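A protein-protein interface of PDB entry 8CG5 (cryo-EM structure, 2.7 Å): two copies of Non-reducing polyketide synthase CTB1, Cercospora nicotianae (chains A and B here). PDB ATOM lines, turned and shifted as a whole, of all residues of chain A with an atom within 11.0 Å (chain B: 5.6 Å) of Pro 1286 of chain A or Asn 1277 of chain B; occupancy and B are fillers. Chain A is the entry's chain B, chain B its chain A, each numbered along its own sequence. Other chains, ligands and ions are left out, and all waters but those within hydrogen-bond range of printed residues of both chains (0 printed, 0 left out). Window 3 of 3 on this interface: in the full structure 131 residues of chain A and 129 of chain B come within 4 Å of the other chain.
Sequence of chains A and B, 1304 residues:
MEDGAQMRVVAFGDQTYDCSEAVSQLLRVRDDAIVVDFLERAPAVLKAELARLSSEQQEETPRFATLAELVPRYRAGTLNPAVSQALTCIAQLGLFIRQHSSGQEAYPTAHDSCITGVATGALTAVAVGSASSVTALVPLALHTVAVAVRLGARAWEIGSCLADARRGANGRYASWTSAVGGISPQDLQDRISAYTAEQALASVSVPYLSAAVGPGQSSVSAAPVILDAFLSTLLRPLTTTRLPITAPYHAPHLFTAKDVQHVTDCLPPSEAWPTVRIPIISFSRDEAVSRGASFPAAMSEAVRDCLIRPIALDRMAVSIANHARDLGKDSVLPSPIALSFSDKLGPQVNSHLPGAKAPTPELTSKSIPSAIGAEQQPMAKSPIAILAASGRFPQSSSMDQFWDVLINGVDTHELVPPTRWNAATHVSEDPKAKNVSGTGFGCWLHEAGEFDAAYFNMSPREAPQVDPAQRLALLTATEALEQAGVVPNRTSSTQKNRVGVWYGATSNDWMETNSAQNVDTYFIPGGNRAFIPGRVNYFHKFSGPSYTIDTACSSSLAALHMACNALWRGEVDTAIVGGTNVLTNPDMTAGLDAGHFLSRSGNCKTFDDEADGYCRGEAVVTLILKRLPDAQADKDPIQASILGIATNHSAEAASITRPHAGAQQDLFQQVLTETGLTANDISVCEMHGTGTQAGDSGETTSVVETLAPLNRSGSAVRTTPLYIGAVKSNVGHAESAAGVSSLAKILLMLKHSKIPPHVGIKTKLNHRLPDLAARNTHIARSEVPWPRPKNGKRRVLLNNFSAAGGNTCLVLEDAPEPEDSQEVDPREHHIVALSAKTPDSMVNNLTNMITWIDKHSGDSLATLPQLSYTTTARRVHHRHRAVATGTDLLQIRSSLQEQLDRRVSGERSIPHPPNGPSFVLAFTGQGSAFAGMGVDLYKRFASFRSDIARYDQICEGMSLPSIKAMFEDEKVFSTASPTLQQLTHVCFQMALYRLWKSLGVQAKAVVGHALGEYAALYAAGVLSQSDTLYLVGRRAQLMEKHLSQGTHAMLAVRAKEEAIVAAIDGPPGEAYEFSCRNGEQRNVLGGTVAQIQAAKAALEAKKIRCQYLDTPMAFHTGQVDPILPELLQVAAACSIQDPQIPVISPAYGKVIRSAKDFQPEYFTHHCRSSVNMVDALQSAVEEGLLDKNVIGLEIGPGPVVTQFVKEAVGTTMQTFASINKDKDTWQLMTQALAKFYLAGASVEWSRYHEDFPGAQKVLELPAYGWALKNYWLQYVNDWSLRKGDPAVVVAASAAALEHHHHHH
The backbone carbonyl oxygen (O) of Asp 1285 of chain A lies within hydrogen-bond range of the guanidinium group (NH2) of Arg 1282 of chain B (2.9 Å).
The side-chain hydroxyl (OH) of Tyr 1275 of chain B lies within hydrogen-bond range of the backbone NH (N) of Trp 1279 of chain B, at 3.4 Å. NH2 of Arg 1282 of chain B sits at hydrogen-bond distance from O of Asn 1277 of chain B (3.1 Å). The side-chain amino group (NZ) of Lys 434 of chain A lies within hydrogen-bond range of the backbone carbonyl oxygen (O) of Lys 1283 of chain A (2.6 Å). The side-chain amino group (NZ) of Lys 434 of chain A is in salt-bridge range of the side-chain carboxylate (OD2) of Asp 1285 of chain A (3.0 Å).
Among the printed residues, pairs that only touch across the chains: Gly 1284 of chain A with Trp 1279 of chain B, Pro 1286 of chain A with Asn 1277 of chain B, Asp 1285 of chain A with Asn 1277 of chain B, Lys 1283 of chain A with Trp 1279 of chain B, Gly 1284 of chain A with Val 1276 of chain B, Pro 1286 of chain A with Arg 1282 of chain B and Gly 1284 of chain A with Asn 1277 of chain B.
Positions printed for both chains: 1279 and 1282. Of the 8 pairs that touch across the chains among the printed residues, none has its exchanged pair printed and touching as well.
Hydrophobic or aromatic side chains of chain A that line the printed part of chain B: Pro 1286. Hydrophobic or aromatic side chains of chain B within 4 Å of the printed part of chain A: Trp 1279. Among the printed residues, 8 pairs touch across the chains. Among the printed residues, no Asp or Glu carboxylate lies within 4 Å of a Lys or Arg side-chain nitrogen of the other chain.
Pro 1286 of chain A touches just these residues of chain B: Asn 1277 and Arg 1282. Of the printed residues of chain A, Asn 1277 of chain B touches Gly 1284, Asp 1285 and Pro 1286. No residue of chain A comes within 4 Å of Tyr 1275 of chain B. Printed residues of chain B within 4 Å of Asp 1285 of chain A: Asn 1277 and Arg 1282. Printed residues of chain A within 4 Å of Arg 1282 of chain B: Asp 1285 and Pro 1286. Printed residues of chain B within 4 Å of Lys 1283 of chain A: Trp 1279. Printed residues of chain B within 4 Å of Gly 1284 of chain A: Val 1276 (3.9 Å), Asn 1277 (3.97 Å) and Trp 1279 (3.2 Å). The nearest printed residue of chain B that does not touch Pro 1286 of chain A is Val 1276 of chain B (6.6 Å). The nearest printed residue of chain B that does not touch Lys 1283 of chain A is Val 1276 of chain B (6.1 Å).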
ATOM      1  N   LYS A 434       6.704  18.057 -11.035  1.00  0.00           N
ATOM      2  CA  LYS A 434       7.408  18.073 -12.308  1.00  0.00           C
ATOM      3  C   LYS A 434       7.179  19.393 -13.035  1.00  0.00           C
ATOM      4  O   LYS A 434       6.044  19.868 -13.144  1.00  0.00           O
ATOM      5  CB  LYS A 434       6.932  16.903 -13.165  1.00  0.00           C
ATOM      6  CG  LYS A 434       7.780  16.620 -14.383  1.00  0.00           C
ATOM      7  CD  LYS A 434       6.918  16.212 -15.565  1.00  0.00           C
ATOM      8  CE  LYS A 434       6.129  14.951 -15.267  1.00  0.00           C
ATOM      9  NZ  LYS A 434       6.279  13.937 -16.342  1.00  0.00           N
ATOM     10  N   TRP A1279      -1.146  21.445 -19.519  1.00  0.00           N
ATOM     11  CA  TRP A1279      -0.561  20.192 -19.977  1.00  0.00           C
ATOM     12  C   TRP A1279       0.960  20.198 -19.949  1.00  0.00           C
ATOM     13  O   TRP A1279       1.565  19.130 -20.079  1.00  0.00           O
ATOM     14  CB  TRP A1279      -1.049  19.866 -21.392  1.00  0.00           C
ATOM     15  CG  TRP A1279      -0.840  20.957 -22.391  1.00  0.00           C
ATOM     16  CD1 TRP A1279      -1.754  21.883 -22.788  1.00  0.00           C
ATOM     17  CD2 TRP A1279       0.352  21.225 -23.133  1.00  0.00           C
ATOM     18  NE1 TRP A1279      -1.204  22.718 -23.727  1.00  0.00           N
ATOM     19  CE2 TRP A1279       0.090  22.334 -23.957  1.00  0.00           C
ATOM     20  CE3 TRP A1279       1.618  20.637 -23.180  1.00  0.00           C
ATOM     21  CZ2 TRP A1279       1.044  22.866 -24.813  1.00  0.00           C
ATOM     22  CZ3 TRP A1279       2.562  21.169 -24.030  1.00  0.00           C
ATOM     23  CH2 TRP A1279       2.271  22.270 -24.835  1.00  0.00           C
ATOM     24  N   LEU A1281       2.716  20.726 -17.345  1.00  0.00           N
ATOM     25  CA  LEU A1281       3.074  20.048 -16.108  1.00  0.00           C
ATOM     26  C   LEU A1281       3.007  18.534 -16.229  1.00  0.00           C
ATOM     27  O   LEU A1281       3.502  17.840 -15.334  1.00  0.00           O
ATOM     28  CB  LEU A1281       2.152  20.499 -14.977  1.00  0.00           C
ATOM     29  CG  LEU A1281       1.939  22.002 -14.807  1.00  0.00           C
ATOM     30  CD1 LEU A1281       1.286  22.283 -13.469  1.00  0.00           C
ATOM     31  CD2 LEU A1281       3.246  22.758 -14.931  1.00  0.00           C
ATOM     32  N   ARG A1282       2.411  18.007 -17.299  1.00  0.00           N
ATOM     33  CA  ARG A1282       2.187  16.573 -17.444  1.00  0.00           C
ATOM     34  C   ARG A1282       2.907  15.996 -18.657  1.00  0.00           C
ATOM     35  O   ARG A1282       2.502  14.951 -19.172  1.00  0.00           O
ATOM     36  CB  ARG A1282       0.688  16.285 -17.533  1.00  0.00           C
ATOM     37  CG  ARG A1282      -0.033  16.401 -16.206  1.00  0.00           C
ATOM     38  CD  ARG A1282      -1.489  16.000 -16.327  1.00  0.00           C
ATOM     39  NE  ARG A1282      -2.297  17.058 -16.923  1.00  0.00           N
ATOM     40  CZ  ARG A1282      -2.626  17.127 -18.205  1.00  0.00           C
ATOM     41  NH1 ARG A1282      -2.226  16.215 -19.075  1.00  0.00           N
ATOM     42  NH2 ARG A1282      -3.375  18.141 -18.627  1.00  0.00           N
ATOM     43  N   LYS A1283       3.965  16.652 -19.125  1.00  0.00           N
ATOM     44  CA  LYS A1283       4.709  16.133 -20.264  1.00  0.00           C
ATOM     45  C   LYS A1283       5.282  14.761 -19.939  1.00  0.00           C
ATOM     46  O   LYS A1283       5.792  14.523 -18.842  1.00  0.00           O
ATOM     47  CB  LYS A1283       5.833  17.092 -20.649  1.00  0.00           C
ATOM     48  CG  LYS A1283       5.368  18.293 -21.442  1.00  0.00           C
ATOM     49  CD  LYS A1283       6.539  19.127 -21.915  1.00  0.00           C
ATOM     50  CE  LYS A1283       6.081  20.255 -22.814  1.00  0.00           C
ATOM     51  NZ  LYS A1283       7.207  20.871 -23.561  1.00  0.00           N
ATOM     52  N   GLY A1284       5.190  13.854 -20.904  1.00  0.00           N
ATOM     53  CA  GLY A1284       5.699  12.508 -20.726  1.00  0.00           C
ATOM     54  C   GLY A1284       4.945  11.701 -19.693  1.00  0.00           C
ATOM     55  O   GLY A1284       5.566  10.974 -18.910  1.00  0.00           O
ATOM     56  N   ASP A1285       3.619  11.809 -19.673  1.00  0.00           N
ATOM     57  CA  ASP A1285       2.791  11.059 -18.744  1.00  0.00           C
ATOM     58  C   ASP A1285       1.605  10.452 -19.474  1.00  0.00           C
ATOM     59  O   ASP A1285       1.173  10.974 -20.506  1.00  0.00           O
ATOM     60  CB  ASP A1285       2.284  11.955 -17.606  1.00  0.00           C
ATOM     61  CG  ASP A1285       3.154  11.873 -16.369  1.00  0.00           C
ATOM     62  OD1 ASP A1285       3.532  10.748 -15.981  1.00  0.00           O
ATOM     63  OD2 ASP A1285       3.458  12.932 -15.782  1.00  0.00           O
ATOM     64  N   PRO A1286       1.050   9.343 -18.957  1.00  0.00           N
ATOM     65  CA  PRO A1286      -0.105   8.694 -19.581  1.00  0.00           C
ATOM     66  C   PRO A1286      -1.437   9.281 -19.129  1.00  0.00           C
ATOM     67  O   PRO A1286      -1.532   9.872 -18.055  1.00  0.00           O
ATOM     68  CB  PRO A1286       0.030   7.247 -19.121  1.00  0.00           C
ATOM     69  CG  PRO A1286       0.675   7.345 -17.780  1.00  0.00           C
ATOM     70  CD  PRO A1286       1.489   8.618 -17.752  1.00  0.00           C
ATOM     71  N   TYR B1275      11.336   9.758 -25.594  1.00  0.00           N
ATOM     72  CA  TYR B1275      10.022  10.386 -25.628  1.00  0.00           C
ATOM     73  C   TYR B1275       8.961   9.303 -25.490  1.00  0.00           C
ATOM     74  O   TYR B1275       8.915   8.370 -26.297  1.00  0.00           O
ATOM     75  CB  TYR B1275       9.844  11.161 -26.929  1.00  0.00           C
ATOM     76  CG  TYR B1275       8.407  11.387 -27.333  1.00  0.00           C
ATOM     77  CD1 TYR B1275       7.618  12.313 -26.673  1.00  0.00           C
ATOM     78  CD2 TYR B1275       7.843  10.683 -28.386  1.00  0.00           C
ATOM     79  CE1 TYR B1275       6.309  12.528 -27.044  1.00  0.00           C
ATOM     80  CE2 TYR B1275       6.533  10.892 -28.762  1.00  0.00           C
ATOM     81  CZ  TYR B1275       5.772  11.815 -28.087  1.00  0.00           C
ATOM     82  OH  TYR B1275       4.466  12.031 -28.453  1.00  0.00           O
ATOM     83  N   VAL B1276       8.108   9.424 -24.474  1.00  0.00           N
ATOM     84  CA  VAL B1276       7.226   8.337 -24.076  1.00  0.00           C
ATOM     85  C   VAL B1276       5.792   8.833 -23.967  1.00  0.00           C
ATOM     86  O   VAL B1276       5.526  10.022 -23.783  1.00  0.00           O
ATOM     87  CB  VAL B1276       7.663   7.706 -22.738  1.00  0.00           C
ATOM     88  CG1 VAL B1276       8.816   6.748 -22.953  1.00  0.00           C
ATOM     89  CG2 VAL B1276       8.039   8.785 -21.739  1.00  0.00           C
ATOM     90  N   ASN B1277       4.865   7.886 -24.090  1.00  0.00           N
ATOM     91  CA  ASN B1277       3.450   8.034 -23.771  1.00  0.00           C
ATOM     92  C   ASN B1277       2.686   8.886 -24.776  1.00  0.00           C
ATOM     93  O   ASN B1277       1.526   9.228 -24.526  1.00  0.00           O
ATOM     94  CB  ASN B1277       3.258   8.604 -22.363  1.00  0.00           C
ATOM     95  CG  ASN B1277       3.300   7.532 -21.300  1.00  0.00           C
ATOM     96  OD1 ASN B1277       4.123   7.578 -20.387  1.00  0.00           O
ATOM     97  ND2 ASN B1277       2.424   6.543 -21.423  1.00  0.00           N
ATOM     98  N   ASP B1278       3.295   9.233 -25.907  1.00  0.00           N
ATOM     99  CA  ASP B1278       2.577   9.846 -27.023  1.00  0.00           C
ATOM    100  C   ASP B1278       1.841  11.113 -26.592  1.00  0.00           C
ATOM    101  O   ASP B1278       0.732  11.393 -27.051  1.00  0.00           O
ATOM    102  CB  ASP B1278       1.596   8.851 -27.644  1.00  0.00           C
ATOM    103  CG  ASP B1278       2.284   7.616 -28.189  1.00  0.00           C
ATOM    104  OD1 ASP B1278       3.045   7.737 -29.169  1.00  0.00           O
ATOM    105  OD2 ASP B1278       2.060   6.520 -27.636  1.00  0.00           O
ATOM    106  N   TRP B1279       2.461  11.892 -25.707  1.00  0.00           N
ATOM    107  CA  TRP B1279       1.795  13.073 -25.173  1.00  0.00           C
ATOM    108  C   TRP B1279       1.691  14.204 -26.187  1.00  0.00           C
ATOM    109  O   TRP B1279       0.958  15.164 -25.936  1.00  0.00           O
ATOM    110  CB  TRP B1279       2.525  13.572 -23.926  1.00  0.00           C
ATOM    111  CG  TRP B1279       3.946  13.957 -24.165  1.00  0.00           C
ATOM    112  CD1 TRP B1279       5.046  13.178 -23.979  1.00  0.00           C
ATOM    113  CD2 TRP B1279       4.426  15.224 -24.625  1.00  0.00           C
ATOM    114  NE1 TRP B1279       6.181  13.879 -24.295  1.00  0.00           N
ATOM    115  CE2 TRP B1279       5.827  15.139 -24.698  1.00  0.00           C
ATOM    116  CE3 TRP B1279       3.806  16.423 -24.987  1.00  0.00           C
ATOM    117  CZ2 TRP B1279       6.617  16.201 -25.116  1.00  0.00           C
ATOM    118  CZ3 TRP B1279       4.593  17.475 -25.402  1.00  0.00           C
ATOM    119  CH2 TRP B1279       5.983  17.358 -25.464  1.00  0.00           C
ATOM    120  N   ARG B1282      -1.898  15.004 -27.600  1.00  0.00           N
ATOM    121  CA  ARG B1282      -2.906  15.471 -26.656  1.00  0.00           C
ATOM    122  C   ARG B1282      -2.494  16.815 -26.076  1.00  0.00           C
ATOM    123  O   ARG B1282      -2.563  17.051 -24.869  1.00  0.00           O
ATOM    124  CB  ARG B1282      -3.115  14.447 -25.548  1.00  0.00           C
ATOM    125  CG  ARG B1282      -3.232  13.020 -26.042  1.00  0.00           C
ATOM    126  CD  ARG B1282      -3.318  12.042 -24.887  1.00  0.00           C
ATOM    127  NE  ARG B1282      -1.997  11.614 -24.441  1.00  0.00           N
ATOM    128  CZ  ARG B1282      -1.655  11.400 -23.179  1.00  0.00           C
ATOM    129  NH1 ARG B1282      -2.518  11.556 -22.188  1.00  0.00           N
ATOM    130  NH2 ARG B1282      -0.413  11.016 -22.901  1.00  0.00           N
